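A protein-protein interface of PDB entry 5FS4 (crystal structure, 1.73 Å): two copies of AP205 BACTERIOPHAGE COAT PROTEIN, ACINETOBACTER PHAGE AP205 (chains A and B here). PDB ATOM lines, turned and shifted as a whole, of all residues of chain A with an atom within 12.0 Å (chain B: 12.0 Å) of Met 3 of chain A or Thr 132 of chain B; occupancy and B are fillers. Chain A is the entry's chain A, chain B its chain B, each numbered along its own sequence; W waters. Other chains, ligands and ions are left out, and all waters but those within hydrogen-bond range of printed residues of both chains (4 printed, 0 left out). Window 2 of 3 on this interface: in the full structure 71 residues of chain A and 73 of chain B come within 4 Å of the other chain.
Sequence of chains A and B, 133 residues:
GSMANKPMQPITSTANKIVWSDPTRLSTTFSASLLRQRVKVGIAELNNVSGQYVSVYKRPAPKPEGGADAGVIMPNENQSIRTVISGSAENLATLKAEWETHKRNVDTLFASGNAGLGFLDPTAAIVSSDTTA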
ATOM      1  N   SER A   2      22.492  27.805  11.986  1.00  0.00           N
ATOM      2  CA  SER A   2      23.317  26.587  11.907  1.00  0.00           C
ATOM      3  C   SER A   2      22.838  25.701  10.757  1.00  0.00           C
ATOM      4  O   SER A   2      21.941  26.089   9.998  1.00  0.00           O
ATOM      5  CB  SER A   2      23.249  25.841  13.229  1.00  0.00           C
ATOM      6  OG  SER A   2      23.253  26.764  14.298  1.00  0.00           O
ATOM      7  N   MET A   3      23.398  24.502  10.642  1.00  0.00           N
ATOM      8  CA  MET A   3      23.264  23.733   9.411  1.00  0.00           C
ATOM      9  C   MET A   3      21.930  22.969   9.236  1.00  0.00           C
ATOM     10  O   MET A   3      21.331  22.444  10.202  1.00  0.00           O
ATOM     11  CB  MET A   3      24.465  22.780   9.271  1.00  0.00           C
ATOM     12  CG  MET A   3      25.813  23.490   9.271  1.00  0.00           C
ATOM     13  SD  MET A   3      25.958  24.748   7.975  1.00  0.00           S
ATOM     14  CE  MET A   3      26.788  23.806   6.683  1.00  0.00           C
ATOM     15  N   ALA A   4      21.474  22.934   7.985  1.00  0.00           N
ATOM     16  CA  ALA A   4      20.419  22.015   7.552  1.00  0.00           C
ATOM     17  C   ALA A   4      20.792  20.546   7.660  1.00  0.00           C
ATOM     18  O   ALA A   4      21.965  20.103   7.515  1.00  0.00           O
ATOM     19  CB  ALA A   4      20.012  22.267   6.112  1.00  0.00           C
ATOM     20  N   ASN A   5      19.738  19.778   7.829  1.00  0.00           N
ATOM     21  CA  ASN A   5      19.858  18.354   7.973  1.00  0.00           C
ATOM     22  C   ASN A   5      20.143  17.818   6.566  1.00  0.00           C
ATOM     23  O   ASN A   5      19.645  18.382   5.567  1.00  0.00           O
ATOM     24  CB  ASN A   5      18.551  17.819   8.543  1.00  0.00           C
ATOM     25  CG  ASN A   5      18.415  18.116  10.006  1.00  0.00           C
ATOM     26  OD1 ASN A   5      18.854  17.316  10.847  1.00  0.00           O
ATOM     27  ND2 ASN A   5      17.882  19.277  10.333  1.00  0.00           N
ATOM     28  N   LYS A   6      20.914  16.737   6.498  1.00  0.00           N
ATOM     29  CA  LYS A   6      21.333  16.162   5.206  1.00  0.00           C
ATOM     30  C   LYS A   6      20.123  15.575   4.479  1.00  0.00           C
ATOM     31  O   LYS A   6      19.347  14.846   5.096  1.00  0.00           O
ATOM     32  CB  LYS A   6      22.415  15.095   5.387  1.00  0.00           C
ATOM     33  CG  LYS A   6      23.720  15.618   5.987  1.00  0.00           C
ATOM     34  CD  LYS A   6      24.781  14.546   6.115  1.00  0.00           C
ATOM     35  CE  LYS A   6      25.273  13.867   4.842  1.00  0.00           C
ATOM     36  NZ  LYS A   6      25.947  12.551   5.142  1.00  0.00           N
ATOM     37  N   PRO A   7      19.956  15.868   3.178  1.00  0.00           N
ATOM     38  CA  PRO A   7      18.788  15.320   2.436  1.00  0.00           C
ATOM     39  C   PRO A   7      19.018  13.879   2.105  1.00  0.00           C
ATOM     40  O   PRO A   7      20.166  13.450   1.884  1.00  0.00           O
ATOM     41  CB  PRO A   7      18.748  16.137   1.144  1.00  0.00           C
ATOM     42  CG  PRO A   7      20.141  16.602   0.937  1.00  0.00           C
ATOM     43  CD  PRO A   7      20.794  16.723   2.311  1.00  0.00           C
ATOM     44  N   MET A   8      17.932  13.123   2.117  1.00  0.00           N
ATOM     45  CA  MET A   8      17.971  11.721   1.758  1.00  0.00           C
ATOM     46  C   MET A   8      17.227  11.536   0.457  1.00  0.00           C
ATOM     47  O   MET A   8      16.276  12.259   0.164  1.00  0.00           O
ATOM     48  CB  MET A   8      17.354  10.879   2.909  1.00  0.00           C
ATOM     49  CG  MET A   8      18.177  10.974   4.212  1.00  0.00           C
ATOM     50  SD  MET A   8      17.468  10.325   5.752  1.00  0.00           S
ATOM     51  CE  MET A   8      17.561   8.640   5.263  1.00  0.00           C
ATOM     52  N   GLN A   9      17.655  10.552  -0.319  1.00  0.00           N
ATOM     53  CA  GLN A   9      17.106  10.327  -1.656  1.00  0.00           C
ATOM     54  C   GLN A   9      16.378   8.982  -1.723  1.00  0.00           C
ATOM     55  O   GLN A   9      16.885   8.029  -1.162  1.00  0.00           O
ATOM     56  CB  GLN A   9      18.263  10.315  -2.671  1.00  0.00           C
ATOM     57  CG  GLN A   9      19.112  11.602  -2.723  1.00  0.00           C
ATOM     58  CD  GLN A   9      18.373  12.877  -3.128  1.00  0.00           C
ATOM     59  OE1 GLN A   9      18.716  13.984  -2.694  1.00  0.00           O
ATOM     60  NE2 GLN A   9      17.348  12.731  -3.961  1.00  0.00           N
ATOM     61  N   SER A  21      17.548   6.884   1.537  1.00  0.00           N
ATOM     62  CA  SER A  21      18.798   6.801   2.220  1.00  0.00           C
ATOM     63  C   SER A  21      19.633   8.043   1.979  1.00  0.00           C
ATOM     64  O   SER A  21      19.438   8.723   1.005  1.00  0.00           O
ATOM     65  CB  SER A  21      19.574   5.571   1.780  1.00  0.00           C
ATOM     66  OG  SER A  21      19.997   5.718   0.450  1.00  0.00           O
ATOM     67  N   ASP A  22      20.523   8.337   2.946  1.00  0.00           N
ATOM     68  CA  ASP A  22      21.567   9.343   2.811  1.00  0.00           C
ATOM     69  C   ASP A  22      22.571   8.890   1.747  1.00  0.00           C
ATOM     70  O   ASP A  22      23.278   7.905   1.941  1.00  0.00           O
ATOM     71  CB  ASP A  22      22.242   9.521   4.170  1.00  0.00           C
ATOM     72  CG  ASP A  22      23.257  10.631   4.202  1.00  0.00           C
ATOM     73  OD1 ASP A  22      23.655  11.124   3.126  1.00  0.00           O
ATOM     74  OD2 ASP A  22      23.689  10.960   5.305  1.00  0.00           O
ATOM     75  N   PRO A  23      22.642   9.599   0.616  1.00  0.00           N
ATOM     76  CA  PRO A  23      23.601   9.147  -0.419  1.00  0.00           C
ATOM     77  C   PRO A  23      25.081   9.164  -0.013  1.00  0.00           C
ATOM     78  O   PRO A  23      25.924   8.552  -0.663  1.00  0.00           O
ATOM     79  CB  PRO A  23      23.336  10.077  -1.606  1.00  0.00           C
ATOM     80  CG  PRO A  23      22.479  11.191  -1.100  1.00  0.00           C
ATOM     81  CD  PRO A  23      21.937  10.837   0.255  1.00  0.00           C
ATOM     82  N   THR A  24      25.419   9.846   1.045  1.00  0.00           N
ATOM     83  CA  THR A  24      26.797   9.740   1.536  1.00  0.00           C
ATOM     84  C   THR A  24      26.915   8.988   2.846  1.00  0.00           C
ATOM     85  O   THR A  24      27.968   9.011   3.441  1.00  0.00           O
ATOM     86  CB  THR A  24      27.443  11.146   1.696  1.00  0.00           C
ATOM     87  OG1 THR A  24      26.718  11.947   2.635  1.00  0.00           O
ATOM     88  CG2 THR A  24      27.515  11.864   0.334  1.00  0.00           C
ATOM     89  N   ARG A  25      25.833   8.358   3.317  1.00  0.00           N
ATOM     90  CA  ARG A  25      25.934   7.394   4.425  1.00  0.00           C
ATOM     91  C   ARG A  25      24.793   6.401   4.251  1.00  0.00           C
ATOM     92  O   ARG A  25      23.724   6.497   4.892  1.00  0.00           O
ATOM     93  CB  ARG A  25      25.937   8.090   5.794  1.00  0.00           C
ATOM     94  CG  ARG A  25      26.350   7.190   6.944  1.00  0.00           C
ATOM     95  CD  ARG A  25      26.124   7.846   8.288  1.00  0.00           C
ATOM     96  NE  ARG A  25      26.464   6.941   9.393  1.00  0.00           N
ATOM     97  CZ  ARG A  25      27.687   6.806   9.911  1.00  0.00           C
ATOM     98  NH1 ARG A  25      28.741   7.490   9.412  1.00  0.00           N
ATOM     99  NH2 ARG A  25      27.876   5.974  10.925  1.00  0.00           N
ATOM    100  N   THR A  28      22.131   4.946   6.583  1.00  0.00           N
ATOM    101  CA  THR A  28      21.108   5.794   7.161  1.00  0.00           C
ATOM    102  C   THR A  28      19.859   5.687   6.296  1.00  0.00           C
ATOM    103  O   THR A  28      19.887   6.021   5.109  1.00  0.00           O
ATOM    104  CB  THR A  28      21.566   7.253   7.324  1.00  0.00           C
ATOM    105  OG1 THR A  28      22.660   7.354   8.251  1.00  0.00           O
ATOM    106  CG2 THR A  28      20.406   8.074   7.882  1.00  0.00           C
ATOM    107  N   TYR A  57      19.823   4.036  11.793  1.00  0.00           N
ATOM    108  CA  TYR A  57      21.122   4.719  11.765  1.00  0.00           C
ATOM    109  C   TYR A  57      22.157   3.767  12.354  1.00  0.00           C
ATOM    110  O   TYR A  57      21.888   3.112  13.349  1.00  0.00           O
ATOM    111  CB  TYR A  57      21.106   6.059  12.522  1.00  0.00           C
ATOM    112  CG  TYR A  57      22.313   6.954  12.237  1.00  0.00           C
ATOM    113  CD1 TYR A  57      23.552   6.680  12.776  1.00  0.00           C
ATOM    114  CD2 TYR A  57      22.189   8.097  11.409  1.00  0.00           C
ATOM    115  CE1 TYR A  57      24.650   7.488  12.495  1.00  0.00           C
ATOM    116  CE2 TYR A  57      23.286   8.864  11.082  1.00  0.00           C
ATOM    117  CZ  TYR A  57      24.516   8.583  11.636  1.00  0.00           C
ATOM    118  OH  TYR A  57      25.616   9.401  11.348  1.00  0.00           O
ATOM    119  N   ALA B  97      18.308  12.348  19.143  1.00  0.00           N
ATOM    120  CA  ALA B  97      18.377  13.085  17.888  1.00  0.00           C
ATOM    121  C   ALA B  97      17.674  12.342  16.751  1.00  0.00           C
ATOM    122  O   ALA B  97      17.042  12.968  15.919  1.00  0.00           O
ATOM    123  CB  ALA B  97      19.827  13.309  17.531  1.00  0.00           C
ATOM    124  N   THR B 101      14.343  13.463  14.524  1.00  0.00           N
ATOM    125  CA  THR B 101      14.360  13.395  13.049  1.00  0.00           C
ATOM    126  C   THR B 101      13.270  12.506  12.503  1.00  0.00           C
ATOM    127  O   THR B 101      12.647  12.837  11.488  1.00  0.00           O
ATOM    128  CB  THR B 101      15.738  12.964  12.537  1.00  0.00           C
ATOM    129  OG1 THR B 101      16.719  13.909  13.023  1.00  0.00           O
ATOM    130  CG2 THR B 101      15.799  12.940  11.044  1.00  0.00           C
ATOM    131  N   ARG B 104      10.021  14.276  12.503  1.00  0.00           N
ATOM    132  CA  ARG B 104      10.030  15.202  11.436  1.00  0.00           C
ATOM    133  C   ARG B 104       9.700  14.539  10.117  1.00  0.00           C
ATOM    134  O   ARG B 104       8.935  15.066   9.332  1.00  0.00           O
ATOM    135  CB  ARG B 104      11.411  15.812  11.341  1.00  0.00           C
ATOM    136  CG  ARG B 104      11.530  16.735  10.152  1.00  0.00           C
ATOM    137  CD  ARG B 104      12.785  17.553  10.245  1.00  0.00           C
ATOM    138  NE  ARG B 104      12.953  18.298   9.011  1.00  0.00           N
ATOM    139  CZ  ARG B 104      14.017  19.035   8.747  1.00  0.00           C
ATOM    140  NH1 ARG B 104      15.039  19.105   9.594  1.00  0.00           N
ATOM    141  NH2 ARG B 104      14.065  19.678   7.595  1.00  0.00           N
ATOM    142  N   ILE B 126      12.684  14.377   2.845  1.00  0.00           N
ATOM    143  CA  ILE B 126      13.138  13.545   3.965  1.00  0.00           C
ATOM    144  C   ILE B 126      14.630  13.815   4.264  1.00  0.00           C
ATOM    145  O   ILE B 126      15.443  14.005   3.334  1.00  0.00           O
ATOM    146  CB  ILE B 126      12.942  12.051   3.610  1.00  0.00           C
ATOM    147  CG1 ILE B 126      11.465  11.721   3.323  1.00  0.00           C
ATOM    148  CG2 ILE B 126      13.511  11.100   4.684  1.00  0.00           C
ATOM    149  CD1 ILE B 126      10.465  12.105   4.425  1.00  0.00           C
ATOM    150  N   VAL B 127      14.968  13.861   5.565  1.00  0.00           N
ATOM    151  CA  VAL B 127      16.275  14.256   5.994  1.00  0.00           C
ATOM    152  C   VAL B 127      16.869  13.334   7.041  1.00  0.00           C
ATOM    153  O   VAL B 127      16.131  12.695   7.781  1.00  0.00           O
ATOM    154  CB  VAL B 127      16.257  15.695   6.557  1.00  0.00           C
ATOM    155  CG1 VAL B 127      15.763  16.667   5.487  1.00  0.00           C
ATOM    156  CG2 VAL B 127      15.432  15.813   7.837  1.00  0.00           C
ATOM    157  N   SER B 128      18.203  13.297   7.088  1.00  0.00           N
ATOM    158  CA  SER B 128      18.929  12.618   8.150  1.00  0.00           C
ATOM    159  C   SER B 128      19.041  13.499   9.354  1.00  0.00           C
ATOM    160  O   SER B 128      18.832  14.677   9.281  1.00  0.00           O
ATOM    161  CB  SER B 128      20.325  12.246   7.646  1.00  0.00           C
ATOM    162  OG  SER B 128      21.159  11.679   8.670  1.00  0.00           O
ATOM    163  N   SER B 129      19.385  12.905  10.483  1.00  0.00           N
ATOM    164  CA  SER B 129      19.686  13.647  11.707  1.00  0.00           C
ATOM    165  C   SER B 129      21.071  14.330  11.586  1.00  0.00           C
ATOM    166  O   SER B 129      21.398  15.246  12.367  1.00  0.00           O
ATOM    167  CB  SER B 129      19.698  12.701  12.866  1.00  0.00           C
ATOM    168  OG  SER B 129      20.653  11.670  12.627  1.00  0.00           O
ATOM    169  N   ASP B 130      21.900  13.830  10.666  1.00  0.00           N
ATOM    170  CA  ASP B 130      23.196  14.459  10.407  1.00  0.00           C
ATOM    171  C   ASP B 130      22.987  15.779   9.709  1.00  0.00           C
ATOM    172  O   ASP B 130      22.017  16.000   8.973  1.00  0.00           O
ATOM    173  CB  ASP B 130      24.110  13.559   9.548  1.00  0.00           C
ATOM    174  CG  ASP B 130      24.685  12.396  10.306  1.00  0.00           C
ATOM    175  OD1 ASP B 130      24.882  12.467  11.536  1.00  0.00           O
ATOM    176  OD2 ASP B 130      25.040  11.419   9.625  1.00  0.00           O
ATOM    177  N   THR B 131      23.922  16.670   9.937  1.00  0.00           N
ATOM    178  CA  THR B 131      23.848  17.994   9.316  1.00  0.00           C
ATOM    179  C   THR B 131      24.965  18.154   8.283  1.00  0.00           C
ATOM    180  O   THR B 131      25.853  17.308   8.152  1.00  0.00           O
ATOM    181  CB  THR B 131      23.844  19.101  10.384  1.00  0.00           C
ATOM    182  OG1 THR B 131      24.871  18.856  11.359  1.00  0.00           O
ATOM    183  CG2 THR B 131      22.479  19.112  11.098  1.00  0.00           C
ATOM    184  N   THR B 132      24.872  19.199   7.478  1.00  0.00           N
ATOM    185  CA  THR B 132      25.754  19.354   6.328  1.00  0.00           C
ATOM    186  C   THR B 132      26.841  20.316   6.788  1.00  0.00           C
ATOM    187  O   THR B 132      28.021  20.132   6.486  1.00  0.00           O
ATOM    188  CB  THR B 132      24.991  19.959   5.141  1.00  0.00           C
ATOM    189  OG1 THR B 132      24.527  21.265   5.523  1.00  0.00           O
ATOM    190  CG2 THR B 132      23.745  19.094   4.718  1.00  0.00           C
HETATM  191  O   HOH W   1      16.816  21.165   7.340  1.00  0.00           O
HETATM  192  O   HOH W   2      14.595  14.248   0.555  1.00  0.00           O
HETATM  193  O   HOH W   3      23.223   9.973   7.774  1.00  0.00           O
HETATM  194  O   HOH W   4      26.893  11.874   7.668  1.00  0.00           O
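OH of Tyr 57 of chain A sits at hydrogen-bond distance from OD2 of Asp 130 of chain B (2.7 Å).
The backbone carbonyl oxygen (O) of Lys 6 of chain A lies within hydrogen-bond range of the backbone NH (N) of Ser 128 of chain B.
The backbone carbonyl oxygen of Asp 130 of chain B lies within hydrogen-bond range of the backbone NH of Lys 6 of chain A (2.8 Å).
The backbone carbonyl oxygen (O) of Val 127 of chain B lies close to the side-chain sulfur (SD) of Met 8 of chain A.
N of Thr 132 of chain B is in hydrogen-bond range of O of Ala 4 of chain A (3.0 Å).
The backbone NH (N) of Met 8 of chain A sits at hydrogen-bond distance from the backbone carbonyl oxygen (O) of Ile 126 of chain B, 2.9 Å away.
OD1 of Asn 5 of chain A lies close to O of Ser 128 of chain B (3.1 Å).
The guanidinium group (NH1) of Arg 104 of chain B sits close to the side-chain amide nitrogen (ND2) of Asn 5 of chain A (2.9 Å).
The side-chain sulfur (SD) of Met 8 of chain A sits at hydrogen-bond distance from the backbone NH (N) of Ser 128 of chain B (3.3 Å).
Among the printed residues, pairs that only touch across the chains: Met 3 of chain A with Thr 131 of chain B (3.6 Å), Met 3 of chain A with Thr 132 of chain B (3.5 Å), Ala 4 of chain A with Thr 131 of chain B (3.4 Å), Asn 5 of chain A with Val 127 of chain B (3.7 Å), Asn 5 of chain A with Ser 129 of chain B (3.6 Å), Asn 5 of chain A with Asp 130 of chain B (3.3 Å), Lys 6 of chain A with Val 127 of chain B (3.3 Å), Lys 6 of chain A with Thr 131 of chain B (3.5 Å), Lys 6 of chain A with Thr 132 of chain B (3.7 Å), Pro 7 of chain A with Ile 126 of chain B (3.7 Å), Arg 25 of chain A with Asp 130 of chain B (3.97 Å) and Thr 28 of chain A with Ser 128 of chain B (3.8 Å).
Met 3 of chain A touches just these residues of chain B: Thr 131 (3.6 Å) and Thr 132 (3.5 Å).
Thr 132 of chain B touches just these residues of chain A: Met 3 (3.5 Å), Ala 4 (3.0 Å) and Lys 6 (3.7 Å).
Ala 4 of chain A touches just these residues of chain B: Thr 131 (3.4 Å) and Thr 132 (3.0 Å).
Printed residues of chain B within 4 Å of Pro 7 of chain A: Ile 126.
Of chain A, only Met 3, Ala 4 and Lys 6 come within 4 Å of Thr 131 of chain B.
Printed residues of chain B within 4 Å of Met 8 of chain A: Ile 126, Val 127 and Ser 128.
Printed residues of chain A within 4 Å of Arg 104 of chain B: Asn 5.
Pro 23 of chain A touches none of the printed residues of chain B.
Of the 10 printed residues of chain B, 8 touch a printed residue of chain A.
Hydrophobic or aromatic side chains of chain B within 4 Å of the printed part of chain A: Val 127.
Printed residues of chain A that touch a printed residue of chain B: Met 3, Ala 4, Asn 5, Lys 6, Pro 7, Met 8, Arg 25, Thr 28 and Tyr 57.
Among the printed residues, 21 pairs touch across the chains.
Among the printed residues, no Asp or Glu carboxylate lies within 4 Å of a Lys or Arg side-chain nitrogen of the other chain.
Water W2 lies within hydrogen-bond range of the backbone carbonyl oxygen (O) of Met 8 of chain A (2.6 Å) and the backbone carbonyl oxygen (O) of Ile 126 of chain B (2.9 Å).
Water W3 lies within hydrogen-bond range of OD2 of Asp 22 of chain A (2.7 Å), OG1 of Thr 28 of chain A (2.7 Å), OG of Ser 128 of chain B (2.8 Å) and OD2 of Asp 130 of chain B (3.0 Å).
Water W4 bridges the side-chain carboxylate of Asp 130 of chain B (2.7 Å) and the side-chain amino group of Lys 6 of chain A (2.8 Å).
Water W1 lies within hydrogen-bond range of NH2 of Arg 104 of chain B (3.1 Å) and N of Asn 5 of chain A (3.3 Å).
No position is printed for both chains.
Of the 21 pairs that touch across the chains among the printed residues, none has its exchanged pair printed and touching as well.
The backbone NH (N) of Asp 22 of chain A lies within hydrogen-bond range of the backbone carbonyl oxygen (O) of Thr 28 of chain A (3.2 Å).
NE of Arg 25 of chain A is in hydrogen-bond range of OH of Tyr 57 of chain A, at 3.3 Å.
N of Asp 130 of chain B is in hydrogen-bond range of OG of Ser 128 of chain B (3.0 Å).
The side-chain carboxylate (OD2) of Asp 22 of chain A is in salt-bridge range of the side-chain amino group (NZ) of Lys 6 of chain A (2.8 Å).
NZ of Lys 6 of chain A sits at hydrogen-bond distance from OG1 of Thr 24 of chain A (2.7 Å).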
